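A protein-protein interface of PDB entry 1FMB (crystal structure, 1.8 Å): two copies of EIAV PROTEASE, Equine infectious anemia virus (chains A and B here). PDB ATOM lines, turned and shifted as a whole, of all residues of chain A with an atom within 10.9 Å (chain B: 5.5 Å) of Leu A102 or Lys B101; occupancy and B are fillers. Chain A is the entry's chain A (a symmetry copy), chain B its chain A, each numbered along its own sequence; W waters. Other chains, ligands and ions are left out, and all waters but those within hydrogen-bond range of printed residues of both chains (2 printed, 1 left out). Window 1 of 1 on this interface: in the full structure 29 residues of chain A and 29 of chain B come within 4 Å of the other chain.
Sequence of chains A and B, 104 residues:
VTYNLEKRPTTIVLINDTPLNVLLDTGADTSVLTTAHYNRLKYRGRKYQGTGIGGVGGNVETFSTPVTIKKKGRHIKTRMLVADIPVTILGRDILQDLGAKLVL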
ATOM      1  N   VAL A   1      12.518  -6.660   4.657  1.00  0.00           N
ATOM      2  CA  VAL A   1      13.980  -6.926   4.548  1.00  0.00           C
ATOM      3  C   VAL A   1      14.181  -7.867   3.358  1.00  0.00           C
ATOM      4  O   VAL A   1      13.272  -8.534   2.891  1.00  0.00           O
ATOM      5  CB  VAL A   1      14.809  -7.457   5.731  1.00  0.00           C
ATOM      6  CG1 VAL A   1      14.713  -6.600   6.996  1.00  0.00           C
ATOM      7  CG2 VAL A   1      14.326  -8.865   6.080  1.00  0.00           C
ATOM      8  N   THR A   2      15.408  -7.837   2.905  1.00  0.00           N
ATOM      9  CA  THR A   2      15.849  -8.570   1.729  1.00  0.00           C
ATOM     10  C   THR A   2      16.883  -9.610   2.083  1.00  0.00           C
ATOM     11  O   THR A   2      17.831  -9.296   2.761  1.00  0.00           O
ATOM     12  CB  THR A   2      16.484  -7.567   0.755  1.00  0.00           C
ATOM     13  OG1 THR A   2      15.410  -6.674   0.328  1.00  0.00           O
ATOM     14  CG2 THR A   2      16.957  -8.277  -0.499  1.00  0.00           C
ATOM     15  N   TYR A   3      16.701 -10.836   1.587  1.00  0.00           N
ATOM     16  CA  TYR A   3      17.663 -11.908   1.815  1.00  0.00           C
ATOM     17  C   TYR A   3      18.283 -12.156   0.446  1.00  0.00           C
ATOM     18  O   TYR A   3      17.564 -12.499  -0.496  1.00  0.00           O
ATOM     19  CB  TYR A   3      16.916 -13.197   2.178  1.00  0.00           C
ATOM     20  CG  TYR A   3      16.225 -13.036   3.514  1.00  0.00           C
ATOM     21  CD1 TYR A   3      14.940 -12.546   3.568  1.00  0.00           C
ATOM     22  CD2 TYR A   3      16.909 -13.466   4.658  1.00  0.00           C
ATOM     23  CE1 TYR A   3      14.346 -12.405   4.804  1.00  0.00           C
ATOM     24  CE2 TYR A   3      16.308 -13.347   5.904  1.00  0.00           C
ATOM     25  CZ  TYR A   3      15.050 -12.785   5.943  1.00  0.00           C
ATOM     26  OH  TYR A   3      14.391 -12.630   7.135  1.00  0.00           O
ATOM     27  N   ASN A   4      19.563 -12.004   0.357  1.00  0.00           N
ATOM     28  CA  ASN A   4      20.381 -12.129  -0.843  1.00  0.00           C
ATOM     29  C   ASN A   4      20.908 -13.549  -1.069  1.00  0.00           C
ATOM     30  O   ASN A   4      21.672 -13.797  -2.017  1.00  0.00           O
ATOM     31  CB  ASN A   4      21.550 -11.144  -0.867  1.00  0.00           C
ATOM     32  CG  ASN A   4      22.668 -11.315   0.168  1.00  0.00           C
ATOM     33  OD1 ASN A   4      22.770 -12.280   0.950  1.00  0.00           O
ATOM     34  ND2 ASN A   4      23.628 -10.383   0.219  1.00  0.00           N
ATOM     35  N   LEU A   5      20.507 -14.436  -0.135  1.00  0.00           N
ATOM     36  CA  LEU A   5      20.825 -15.862  -0.255  1.00  0.00           C
ATOM     37  C   LEU A   5      22.243 -16.317  -0.123  1.00  0.00           C
ATOM     38  O   LEU A   5      22.552 -17.501  -0.298  1.00  0.00           O
ATOM     39  CB  LEU A   5      20.088 -16.482  -1.482  1.00  0.00           C
ATOM     40  CG  LEU A   5      18.639 -16.054  -1.666  1.00  0.00           C
ATOM     41  CD1 LEU A   5      18.035 -16.440  -3.028  1.00  0.00           C
ATOM     42  CD2 LEU A   5      17.777 -16.568  -0.537  1.00  0.00           C
ATOM     43  N   GLU A   6      23.134 -15.447   0.404  1.00  0.00           N
ATOM     44  CA  GLU A   6      24.487 -15.832   0.789  1.00  0.00           C
ATOM     45  C   GLU A   6      24.402 -16.797   1.993  1.00  0.00           C
ATOM     46  O   GLU A   6      25.281 -17.647   2.135  1.00  0.00           O
ATOM     47  CB  GLU A   6      25.259 -14.648   1.361  1.00  0.00           C
ATOM     48  CG  GLU A   6      25.749 -13.859   0.132  1.00  0.00           C
ATOM     49  CD  GLU A   6      26.112 -12.464   0.677  1.00  0.00           C
ATOM     50  OE1 GLU A   6      25.777 -12.257   1.873  1.00  0.00           O
ATOM     51  OE2 GLU A   6      26.664 -11.740  -0.160  1.00  0.00           O
ATOM     52  N   LYS A   7      23.369 -16.627   2.796  1.00  0.00           N
ATOM     53  CA  LYS A   7      23.171 -17.537   3.945  1.00  0.00           C
ATOM     54  C   LYS A   7      21.763 -18.087   3.887  1.00  0.00           C
ATOM     55  O   LYS A   7      20.905 -17.641   3.068  1.00  0.00           O
ATOM     56  CB  LYS A   7      23.523 -16.814   5.244  1.00  0.00           C
ATOM     57  CG  LYS A   7      25.067 -16.718   5.277  1.00  0.00           C
ATOM     58  CD  LYS A   7      25.482 -16.473   6.717  1.00  0.00           C
ATOM     59  CE  LYS A   7      26.966 -16.747   6.910  1.00  0.00           C
ATOM     60  NZ  LYS A   7      27.426 -16.049   8.161  1.00  0.00           N
ATOM     61  N   PRO A   9      18.035 -18.246   4.427  1.00  0.00           N
ATOM     62  CA  PRO A   9      17.135 -17.151   4.830  1.00  0.00           C
ATOM     63  C   PRO A   9      16.285 -17.624   6.017  1.00  0.00           C
ATOM     64  O   PRO A   9      15.265 -18.330   5.960  1.00  0.00           O
ATOM     65  CB  PRO A   9      16.327 -16.932   3.540  1.00  0.00           C
ATOM     66  CG  PRO A   9      16.353 -18.234   2.822  1.00  0.00           C
ATOM     67  CD  PRO A   9      17.629 -18.953   3.177  1.00  0.00           C
ATOM     68  N   LEU A  24      12.795 -19.764   5.576  1.00  0.00           N
ATOM     69  CA  LEU A  24      11.816 -19.225   4.619  1.00  0.00           C
ATOM     70  C   LEU A  24      12.110 -19.979   3.298  1.00  0.00           C
ATOM     71  O   LEU A  24      13.168 -19.818   2.665  1.00  0.00           O
ATOM     72  CB  LEU A  24      12.082 -17.735   4.391  1.00  0.00           C
ATOM     73  CG  LEU A  24      12.083 -17.012   5.776  1.00  0.00           C
ATOM     74  CD1 LEU A  24      12.395 -15.530   5.577  1.00  0.00           C
ATOM     75  CD2 LEU A  24      10.739 -17.232   6.383  1.00  0.00           C
ATOM     76  N   ASP A  25      11.195 -20.853   2.971  1.00  0.00           N
ATOM     77  CA  ASP A  25      11.422 -21.802   1.880  1.00  0.00           C
ATOM     78  C   ASP A  25      10.455 -21.790   0.712  1.00  0.00           C
ATOM     79  O   ASP A  25       9.330 -22.305   0.767  1.00  0.00           O
ATOM     80  CB  ASP A  25      11.432 -23.194   2.566  1.00  0.00           C
ATOM     81  CG  ASP A  25      11.855 -24.368   1.679  1.00  0.00           C
ATOM     82  OD1 ASP A  25      12.184 -24.095   0.497  1.00  0.00           O
ATOM     83  OD2 ASP A  25      11.707 -25.471   2.221  1.00  0.00           O
ATOM     84  N   THR A  26      10.953 -21.179  -0.375  1.00  0.00           N
ATOM     85  CA  THR A  26      10.080 -21.125  -1.592  1.00  0.00           C
ATOM     86  C   THR A  26       9.891 -22.503  -2.237  1.00  0.00           C
ATOM     87  O   THR A  26       8.985 -22.569  -3.094  1.00  0.00           O
ATOM     88  CB  THR A  26      10.610 -20.170  -2.669  1.00  0.00           C
ATOM     89  OG1 THR A  26      11.941 -20.591  -3.044  1.00  0.00           O
ATOM     90  CG2 THR A  26      10.795 -18.773  -2.077  1.00  0.00           C
ATOM     91  N   GLY A  27      10.701 -23.509  -1.961  1.00  0.00           N
ATOM     92  CA  GLY A  27      10.518 -24.839  -2.509  1.00  0.00           C
ATOM     93  C   GLY A  27       9.616 -25.702  -1.661  1.00  0.00           C
ATOM     94  O   GLY A  27       9.505 -26.883  -1.947  1.00  0.00           O
ATOM     95  N   ALA A  28       8.926 -25.235  -0.619  1.00  0.00           N
ATOM     96  CA  ALA A  28       8.053 -26.027   0.232  1.00  0.00           C
ATOM     97  C   ALA A  28       6.634 -25.562  -0.048  1.00  0.00           C
ATOM     98  O   ALA A  28       6.363 -24.342  -0.002  1.00  0.00           O
ATOM     99  CB  ALA A  28       8.435 -25.856   1.720  1.00  0.00           C
ATOM    100  N   LYS A  72       5.836  -9.440  11.459  1.00  0.00           N
ATOM    101  CA  LYS A  72       5.541  -8.275  10.604  1.00  0.00           C
ATOM    102  C   LYS A  72       4.204  -7.673  11.044  1.00  0.00           C
ATOM    103  O   LYS A  72       3.361  -7.296  10.227  1.00  0.00           O
ATOM    104  CB  LYS A  72       5.339  -8.811   9.191  1.00  0.00           C
ATOM    105  CG  LYS A  72       6.398  -8.710   8.135  1.00  0.00           C
ATOM    106  CD  LYS A  72       5.706  -9.067   6.816  1.00  0.00           C
ATOM    107  CE  LYS A  72       5.973  -7.956   5.795  1.00  0.00           C
ATOM    108  NZ  LYS A  72       5.636  -8.308   4.385  1.00  0.00           N
ATOM    109  N   ARG A  92       5.258 -21.847   1.125  1.00  0.00           N
ATOM    110  CA  ARG A  92       4.496 -20.899   0.302  1.00  0.00           C
ATOM    111  C   ARG A  92       3.149 -20.504   0.868  1.00  0.00           C
ATOM    112  O   ARG A  92       2.726 -19.358   0.644  1.00  0.00           O
ATOM    113  CB  ARG A  92       4.401 -21.427  -1.154  1.00  0.00           C
ATOM    114  CG  ARG A  92       5.792 -21.462  -1.868  1.00  0.00           C
ATOM    115  CD  ARG A  92       5.506 -21.732  -3.388  1.00  0.00           C
ATOM    116  NE  ARG A  92       4.884 -23.019  -3.642  1.00  0.00           N
ATOM    117  CZ  ARG A  92       3.603 -23.304  -3.834  1.00  0.00           C
ATOM    118  NH1 ARG A  92       2.645 -22.337  -3.885  1.00  0.00           N
ATOM    119  NH2 ARG A  92       3.149 -24.547  -4.041  1.00  0.00           N
ATOM    120  N   LEU A  95       4.221 -17.967   3.522  1.00  0.00           N
ATOM    121  CA  LEU A  95       4.938 -16.882   2.880  1.00  0.00           C
ATOM    122  C   LEU A  95       3.987 -15.949   2.112  1.00  0.00           C
ATOM    123  O   LEU A  95       4.198 -14.744   2.086  1.00  0.00           O
ATOM    124  CB  LEU A  95       5.983 -17.473   1.927  1.00  0.00           C
ATOM    125  CG  LEU A  95       7.206 -18.076   2.609  1.00  0.00           C
ATOM    126  CD1 LEU A  95       8.204 -18.594   1.582  1.00  0.00           C
ATOM    127  CD2 LEU A  95       7.908 -17.164   3.611  1.00  0.00           C
ATOM    128  N   GLN A  96       2.981 -16.486   1.426  1.00  0.00           N
ATOM    129  CA  GLN A  96       1.985 -15.741   0.663  1.00  0.00           C
ATOM    130  C   GLN A  96       1.200 -14.863   1.634  1.00  0.00           C
ATOM    131  O   GLN A  96       0.970 -13.647   1.422  1.00  0.00           O
ATOM    132  CB  GLN A  96       1.061 -16.694  -0.095  1.00  0.00           C
ATOM    133  CG  GLN A  96       0.053 -16.016  -1.001  1.00  0.00           C
ATOM    134  CD  GLN A  96      -0.864 -16.973  -1.753  1.00  0.00           C
ATOM    135  OE1 GLN A  96      -0.670 -18.184  -1.712  1.00  0.00           O
ATOM    136  NE2 GLN A  96      -1.876 -16.439  -2.432  1.00  0.00           N
ATOM    137  N   LEU A  98       2.225 -13.674   4.530  1.00  0.00           N
ATOM    138  CA  LEU A  98       3.090 -12.645   4.997  1.00  0.00           C
ATOM    139  C   LEU A  98       3.454 -11.663   3.872  1.00  0.00           C
ATOM    140  O   LEU A  98       4.104 -10.663   4.229  1.00  0.00           O
ATOM    141  CB  LEU A  98       4.433 -13.103   5.611  1.00  0.00           C
ATOM    142  CG  LEU A  98       4.242 -13.890   6.919  1.00  0.00           C
ATOM    143  CD1 LEU A  98       5.513 -14.596   7.356  1.00  0.00           C
ATOM    144  CD2 LEU A  98       3.790 -12.951   8.031  1.00  0.00           C
ATOM    145  N   GLY A  99       3.127 -11.867   2.618  1.00  0.00           N
ATOM    146  CA  GLY A  99       3.522 -10.894   1.607  1.00  0.00           C
ATOM    147  C   GLY A  99       4.924 -11.132   1.103  1.00  0.00           C
ATOM    148  O   GLY A  99       5.472 -10.239   0.476  1.00  0.00           O
ATOM    149  N   ALA A 100       5.583 -12.276   1.317  1.00  0.00           N
ATOM    150  CA  ALA A 100       6.949 -12.493   0.853  1.00  0.00           C
ATOM    151  C   ALA A 100       6.970 -12.638  -0.666  1.00  0.00           C
ATOM    152  O   ALA A 100       5.978 -13.015  -1.258  1.00  0.00           O
ATOM    153  CB  ALA A 100       7.522 -13.827   1.365  1.00  0.00           C
ATOM    154  N   LYS A 101       8.037 -12.238  -1.309  1.00  0.00           N
ATOM    155  CA  LYS A 101       8.063 -12.398  -2.773  1.00  0.00           C
ATOM    156  C   LYS A 101       9.486 -12.772  -3.160  1.00  0.00           C
ATOM    157  O   LYS A 101      10.452 -12.367  -2.520  1.00  0.00           O
ATOM    158  CB  LYS A 101       7.602 -11.109  -3.459  1.00  0.00           C
ATOM    159  CG  LYS A 101       8.584  -9.981  -3.187  1.00  0.00           C
ATOM    160  CD  LYS A 101       8.193  -8.673  -3.858  1.00  0.00           C
ATOM    161  CE  LYS A 101       6.748  -8.336  -3.513  1.00  0.00           C
ATOM    162  NZ  LYS A 101       6.494  -6.887  -3.782  1.00  0.00           N
ATOM    163  N   LEU A 102       9.676 -13.558  -4.222  1.00  0.00           N
ATOM    164  CA  LEU A 102      11.011 -13.892  -4.673  1.00  0.00           C
ATOM    165  C   LEU A 102      11.219 -13.064  -5.983  1.00  0.00           C
ATOM    166  O   LEU A 102      10.291 -13.108  -6.826  1.00  0.00           O
ATOM    167  CB  LEU A 102      11.030 -15.383  -5.182  1.00  0.00           C
ATOM    168  CG  LEU A 102      12.358 -15.882  -5.666  1.00  0.00           C
ATOM    169  CD1 LEU A 102      13.453 -15.869  -4.609  1.00  0.00           C
ATOM    170  CD2 LEU A 102      12.327 -17.388  -6.015  1.00  0.00           C
ATOM    171  N   VAL A 103      12.314 -12.363  -6.074  1.00  0.00           N
ATOM    172  CA  VAL A 103      12.596 -11.538  -7.239  1.00  0.00           C
ATOM    173  C   VAL A 103      13.784 -12.101  -7.998  1.00  0.00           C
ATOM    174  O   VAL A 103      14.857 -12.197  -7.421  1.00  0.00           O
ATOM    175  CB  VAL A 103      13.032 -10.130  -6.843  1.00  0.00           C
ATOM    176  CG1 VAL A 103      13.125  -9.106  -7.966  1.00  0.00           C
ATOM    177  CG2 VAL A 103      12.013  -9.578  -5.853  1.00  0.00           C
ATOM    178  N   LEU A 104      13.528 -12.340  -9.277  1.00  0.00           N
ATOM    179  CA  LEU A 104      14.621 -12.833 -10.102  1.00  0.00           C
ATOM    180  C   LEU A 104      14.772 -11.788 -11.218  1.00  0.00           C
ATOM    181  O   LEU A 104      15.740 -11.002 -11.287  1.00  0.00           O
ATOM    182  CB  LEU A 104      14.298 -14.214 -10.628  1.00  0.00           C
ATOM    183  CG  LEU A 104      15.493 -15.046 -11.114  1.00  0.00           C
ATOM    184  CD1 LEU A 104      15.138 -15.668 -12.451  1.00  0.00           C
ATOM    185  CD2 LEU A 104      16.784 -14.249 -11.266  1.00  0.00           C
ATOM    186  OXT LEU A 104      13.848 -11.777 -12.055  1.00  0.00           O
ATOM    187  N   VAL B   1      11.599 -10.368 -12.725  1.00  0.00           N
ATOM    188  CA  VAL B   1      10.176 -10.735 -12.483  1.00  0.00           C
ATOM    189  C   VAL B   1      10.056 -11.137 -11.011  1.00  0.00           C
ATOM    190  O   VAL B   1      11.025 -11.450 -10.338  1.00  0.00           O
ATOM    191  CB  VAL B   1       9.444 -11.789 -13.333  1.00  0.00           C
ATOM    192  CG1 VAL B   1       9.470 -11.507 -14.838  1.00  0.00           C
ATOM    193  CG2 VAL B   1      10.094 -13.152 -13.100  1.00  0.00           C
ATOM    194  N   THR B   2       8.823 -11.071 -10.578  1.00  0.00           N
ATOM    195  CA  THR B   2       8.442 -11.317  -9.197  1.00  0.00           C
ATOM    196  C   THR B   2       7.545 -12.523  -9.079  1.00  0.00           C
ATOM    197  O   THR B   2       6.584 -12.619  -9.803  1.00  0.00           O
ATOM    198  CB  THR B   2       7.671 -10.087  -8.691  1.00  0.00           C
ATOM    199  OG1 THR B   2       8.624  -8.981  -8.685  1.00  0.00           O
ATOM    200  CG2 THR B   2       7.254 -10.285  -7.246  1.00  0.00           C
ATOM    201  N   TYR B   3       7.856 -13.417  -8.137  1.00  0.00           N
ATOM    202  CA  TYR B   3       7.031 -14.594  -7.893  1.00  0.00           C
ATOM    203  C   TYR B   3       6.411 -14.343  -6.525  1.00  0.00           C
ATOM    204  O   TYR B   3       7.141 -14.193  -5.542  1.00  0.00           O
ATOM    205  CB  TYR B   3       7.931 -15.824  -7.727  1.00  0.00           C
ATOM    206  CG  TYR B   3       8.631 -16.134  -9.031  1.00  0.00           C
ATOM    207  CD1 TYR B   3       9.851 -15.561  -9.308  1.00  0.00           C
ATOM    208  CD2 TYR B   3       8.030 -17.062  -9.890  1.00  0.00           C
ATOM    209  CE1 TYR B   3      10.455 -15.860 -10.512  1.00  0.00           C
ATOM    210  CE2 TYR B   3       8.643 -17.384 -11.094  1.00  0.00           C
ATOM    211  CZ  TYR B   3       9.828 -16.744 -11.385  1.00  0.00           C
ATOM    212  OH  TYR B   3      10.494 -17.004 -12.555  1.00  0.00           O
ATOM    213  N   ASN B   4       5.120 -14.317  -6.473  1.00  0.00           N
ATOM    214  CA  ASN B   4       4.292 -14.045  -5.303  1.00  0.00           C
ATOM    215  C   ASN B   4       3.929 -15.306  -4.515  1.00  0.00           C
ATOM    216  O   ASN B   4       3.176 -15.240  -3.528  1.00  0.00           O
ATOM    217  CB  ASN B   4       3.017 -13.276  -5.648  1.00  0.00           C
ATOM    218  CG  ASN B   4       1.952 -13.976  -6.500  1.00  0.00           C
ATOM    219  OD1 ASN B   4       1.982 -15.178  -6.827  1.00  0.00           O
ATOM    220  ND2 ASN B   4       0.892 -13.261  -6.898  1.00  0.00           N
ATOM    221  N   LEU B   5       4.453 -16.440  -5.024  1.00  0.00           N
ATOM    222  CA  LEU B   5       4.299 -17.725  -4.334  1.00  0.00           C
ATOM    223  C   LEU B   5       2.948 -18.355  -4.238  1.00  0.00           C
ATOM    224  O   LEU B   5       2.775 -19.397  -3.596  1.00  0.00           O
ATOM    225  CB  LEU B   5       5.074 -17.710  -2.980  1.00  0.00           C
ATOM    226  CG  LEU B   5       6.458 -17.080  -3.019  1.00  0.00           C
ATOM    227  CD1 LEU B   5       7.070 -16.813  -1.631  1.00  0.00           C
ATOM    228  CD2 LEU B   5       7.402 -17.899  -3.867  1.00  0.00           C
ATOM    229  N   PRO B   9       7.461 -21.445  -7.734  1.00  0.00           N
ATOM    230  CA  PRO B   9       8.237 -20.506  -8.564  1.00  0.00           C
ATOM    231  C   PRO B   9       9.165 -21.313  -9.483  1.00  0.00           C
ATOM    232  O   PRO B   9      10.259 -21.814  -9.171  1.00  0.00           O
ATOM    233  CB  PRO B   9       8.983 -19.697  -7.490  1.00  0.00           C
ATOM    234  CG  PRO B   9       9.091 -20.595  -6.310  1.00  0.00           C
ATOM    235  CD  PRO B   9       7.915 -21.539  -6.316  1.00  0.00           C
ATOM    236  N   LEU B  24      12.868 -22.676  -8.305  1.00  0.00           N
ATOM    237  CA  LEU B  24      13.755 -21.689  -7.669  1.00  0.00           C
ATOM    238  C   LEU B  24      13.518 -21.878  -6.150  1.00  0.00           C
ATOM    239  O   LEU B  24      12.434 -21.601  -5.609  1.00  0.00           O
ATOM    240  CB  LEU B  24      13.312 -20.274  -8.051  1.00  0.00           C
ATOM    241  CG  LEU B  24      13.260 -20.172  -9.610  1.00  0.00           C
ATOM    242  CD1 LEU B  24      12.774 -18.782 -10.014  1.00  0.00           C
ATOM    243  CD2 LEU B  24      14.636 -20.460 -10.110  1.00  0.00           C
ATOM    244  N   THR B  26      14.717 -21.362  -2.333  1.00  0.00           N
ATOM    245  CA  THR B  26      15.547 -20.723  -1.262  1.00  0.00           C
ATOM    246  C   THR B  26      15.880 -21.695  -0.123  1.00  0.00           C
ATOM    247  O   THR B  26      16.766 -21.305   0.666  1.00  0.00           O
ATOM    248  CB  THR B  26      14.884 -19.485  -0.645  1.00  0.00           C
ATOM    249  OG1 THR B  26      13.602 -19.872  -0.101  1.00  0.00           O
ATOM    250  CG2 THR B  26      14.553 -18.474  -1.744  1.00  0.00           C
ATOM    251  N   LEU B  95      21.123 -19.223  -7.354  1.00  0.00           N
ATOM    252  CA  LEU B  95      20.269 -18.063  -7.184  1.00  0.00           C
ATOM    253  C   LEU B  95      21.087 -16.798  -6.877  1.00  0.00           C
ATOM    254  O   LEU B  95      20.737 -15.717  -7.332  1.00  0.00           O
ATOM    255  CB  LEU B  95      19.277 -18.340  -6.049  1.00  0.00           C
ATOM    256  CG  LEU B  95      18.149 -19.303  -6.401  1.00  0.00           C
ATOM    257  CD1 LEU B  95      17.194 -19.478  -5.229  1.00  0.00           C
ATOM    258  CD2 LEU B  95      17.371 -18.957  -7.667  1.00  0.00           C
ATOM    259  N   GLY B  99      21.479 -13.191  -8.999  1.00  0.00           N
ATOM    260  CA  GLY B  99      20.949 -11.947  -8.454  1.00  0.00           C
ATOM    261  C   GLY B  99      19.572 -12.125  -7.863  1.00  0.00           C
ATOM    262  O   GLY B  99      18.909 -11.125  -7.633  1.00  0.00           O
ATOM    263  N   ALA B 100      19.056 -13.326  -7.583  1.00  0.00           N
ATOM    264  CA  ALA B 100      17.713 -13.496  -7.038  1.00  0.00           C
ATOM    265  C   ALA B 100      17.672 -13.021  -5.589  1.00  0.00           C
ATOM    266  O   ALA B 100      18.687 -13.011  -4.920  1.00  0.00           O
ATOM    267  CB  ALA B 100      17.312 -14.980  -6.959  1.00  0.00           C
ATOM    268  N   LYS B 101      16.551 -12.524  -5.135  1.00  0.00           N
ATOM    269  CA  LYS B 101      16.508 -12.085  -3.729  1.00  0.00           C
ATOM    270  C   LYS B 101      15.129 -12.435  -3.190  1.00  0.00           C
ATOM    271  O   LYS B 101      14.139 -12.436  -3.915  1.00  0.00           O
ATOM    272  CB  LYS B 101      16.800 -10.585  -3.629  1.00  0.00           C
ATOM    273  CG  LYS B 101      15.700  -9.783  -4.306  1.00  0.00           C
ATOM    274  CD  LYS B 101      15.920  -8.280  -4.225  1.00  0.00           C
ATOM    275  CE  LYS B 101      17.324  -7.944  -4.713  1.00  0.00           C
ATOM    276  NZ  LYS B 101      17.402  -6.490  -5.053  1.00  0.00           N
ATOM    277  N   LEU B 102      15.005 -12.745  -1.897  1.00  0.00           N
ATOM    278  CA  LEU B 102      13.708 -13.023  -1.317  1.00  0.00           C
ATOM    279  C   LEU B 102      13.373 -11.770  -0.445  1.00  0.00           C
ATOM    280  O   LEU B 102      14.280 -11.364   0.321  1.00  0.00           O
ATOM    281  CB  LEU B 102      13.850 -14.176  -0.253  1.00  0.00           C
ATOM    282  CG  LEU B 102      12.578 -14.589   0.423  1.00  0.00           C
ATOM    283  CD1 LEU B 102      11.514 -15.129  -0.524  1.00  0.00           C
ATOM    284  CD2 LEU B 102      12.775 -15.814   1.345  1.00  0.00           C
ATOM    285  N   VAL B 103      12.202 -11.223  -0.616  1.00  0.00           N
ATOM    286  CA  VAL B 103      11.798 -10.039   0.127  1.00  0.00           C
ATOM    287  C   VAL B 103      10.666 -10.384   1.076  1.00  0.00           C
ATOM    288  O   VAL B 103       9.625 -10.828   0.612  1.00  0.00           O
ATOM    289  CB  VAL B 103      11.211  -8.969  -0.790  1.00  0.00           C
ATOM    290  CG1 VAL B 103      10.973  -7.599  -0.170  1.00  0.00           C
ATOM    291  CG2 VAL B 103      12.184  -8.746  -1.943  1.00  0.00           C
HETATM  292  O   HOH W   1      21.430 -12.572  -4.382  1.00  0.00           O
HETATM  293  O   HOH W   2       3.216 -13.151  -1.860  1.00  0.00           O
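N of Leu B24 sits at hydrogen-bond distance from O of Pro B9 (2.9 Å).
The backbone carbonyl oxygen (O) of Leu B95 sits at hydrogen-bond distance from the backbone NH (N) of Ala B100 (2.9 Å).
N of Leu A24 sits at hydrogen-bond distance from O of Pro A9.
The backbone carbonyl oxygen of Ala A28 sits at hydrogen-bond distance from the backbone NH of Arg A92, 3.0 Å away.
O of Leu A95 lies within hydrogen-bond range of N of Ala A100, at 2.9 Å.
Tyr A3 touches Lys B101, and with the chains exchanged Lys A101 touches Tyr B3.
Leu A5 touches Thr B26, and with the chains exchanged Thr A26 touches Leu B5.
Leu A5 touches Ala B100, and with the chains exchanged Ala A100 touches Leu B5.
Ala A100 touches Val B103, and with the chains exchanged Val A103 touches Ala B100.
Positions printed for both chains: 1, 2, 3, 4, 5, 9, 24, 26, 95, 99, 100, 101, 102 and 103.
Hydrophobic or aromatic side chains of chain B within 4 Å of the printed part of chain A: Tyr B3, Leu B5, Pro B9, Leu B24, Leu B95, Ala B100, Leu B102 and Val B103.
Hydrophobic or aromatic side chains of chain A within 4 Å of the printed part of chain B: Tyr A3, Leu A5, Pro A9, Leu A24, Leu A95, Ala A100, Leu A102 and Val A103.
Among the printed residues, 36 pairs touch across the chains.
Among the printed residues, no Asp or Glu carboxylate lies within 4 Å of a Lys or Arg side-chain nitrogen of the other chain.
The backbone NH (N) of Val B1 sits at hydrogen-bond distance from the chain-end carboxylate (OXT) of Leu A104 (2.7 Å).
The backbone NH of Tyr B3 sits at hydrogen-bond distance from the backbone carbonyl oxygen of Leu A102 (2.8 Å).
The backbone carbonyl oxygen (O) of Leu B5 lies within hydrogen-bond range of the guanidinium group (NH1) of Arg A92, 3.0 Å away.
The side-chain hydroxyl (OG1) of Thr A26 is in hydrogen-bond range of the backbone carbonyl oxygen (O) of Leu B24, at 2.8 Å.
The backbone carbonyl oxygen (O) of Leu A24 is in hydrogen-bond range of the side-chain hydroxyl (OG1) of Thr B26 (2.8 Å).
The side-chain hydroxyl of Thr A26 is in hydrogen-bond range of the backbone NH of Thr B26, at 3.0 Å.
The backbone carbonyl oxygen (O) of Lys B101 sits at hydrogen-bond distance from the backbone NH (N) of Val A103, 2.8 Å away.
The backbone carbonyl oxygen (O) of Leu B102 sits at hydrogen-bond distance from the backbone NH (N) of Tyr A3 (2.8 Å).
The backbone carbonyl oxygen (O) of Lys A101 lies within hydrogen-bond range of the backbone NH (N) of Val B103, 2.8 Å away.
Of the printed residues of chain A, Pro B9 touches Thr A26 (3.5 Å) and Arg A92 (3.8 Å).
Leu B24 touches just these residues of chain A: Thr A26 and Leu A102.
Of the printed residues of chain B, Leu A5 touches Thr B26 (3.9 Å), Leu B95 (3.8 Å) and Ala B100 (3.97 Å).
Printed residues of chain B within 4 Å of Lys A101: Thr B2 (3.9 Å), Tyr B3 (3.4 Å), Lys B101 (3.9 Å), Leu B102 (3.5 Å) and Val B103 (2.8 Å).
Of the printed residues of chain B, Asp A25 touches Thr B26 (3.5 Å).
Glu A6 touches none of the printed residues of chain B.
The nearest printed residue of chain A that does not touch Lys B101 is Leu A5 (4.7 Å).
Among the printed residues, merely in contact across the chains: Val A1 with Leu B102, Val A1 with Val B103, Thr A2 with Lys B101, Thr A2 with Leu B102, Tyr A3 with Lys B101, Leu A5 with Thr B26, Leu A5 with Leu B95, Leu A5 with Ala B100, Pro A9 with Thr B26, Leu A24 with Leu B102, Asp A25 with Thr B26, Thr A26 with Leu B5, Thr A26 with Pro B9, Arg A92 with Pro B9, Leu A95 with Leu B5, Ala A100 with Leu B5, Ala A100 with Val B103, Lys A101 with Thr B2, Lys A101 with Tyr B3, Lys A101 with Lys B101, Lys A101 with Leu B102, Leu A102 with Val B1, Leu A102 with Thr B2, Leu A102 with Leu B24, Leu A102 with Lys B101, Val A103 with Val B1 and Val A103 with Ala B100.
Water W1 lies within hydrogen-bond range of the backbone carbonyl oxygen (O) of Asn A4 (2.7 Å) and the backbone carbonyl oxygen (O) of Ala B100 (2.8 Å).
Water W2 bridges O of Asn B4 (2.7 Å) and O of Ala A100 (2.8 Å).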
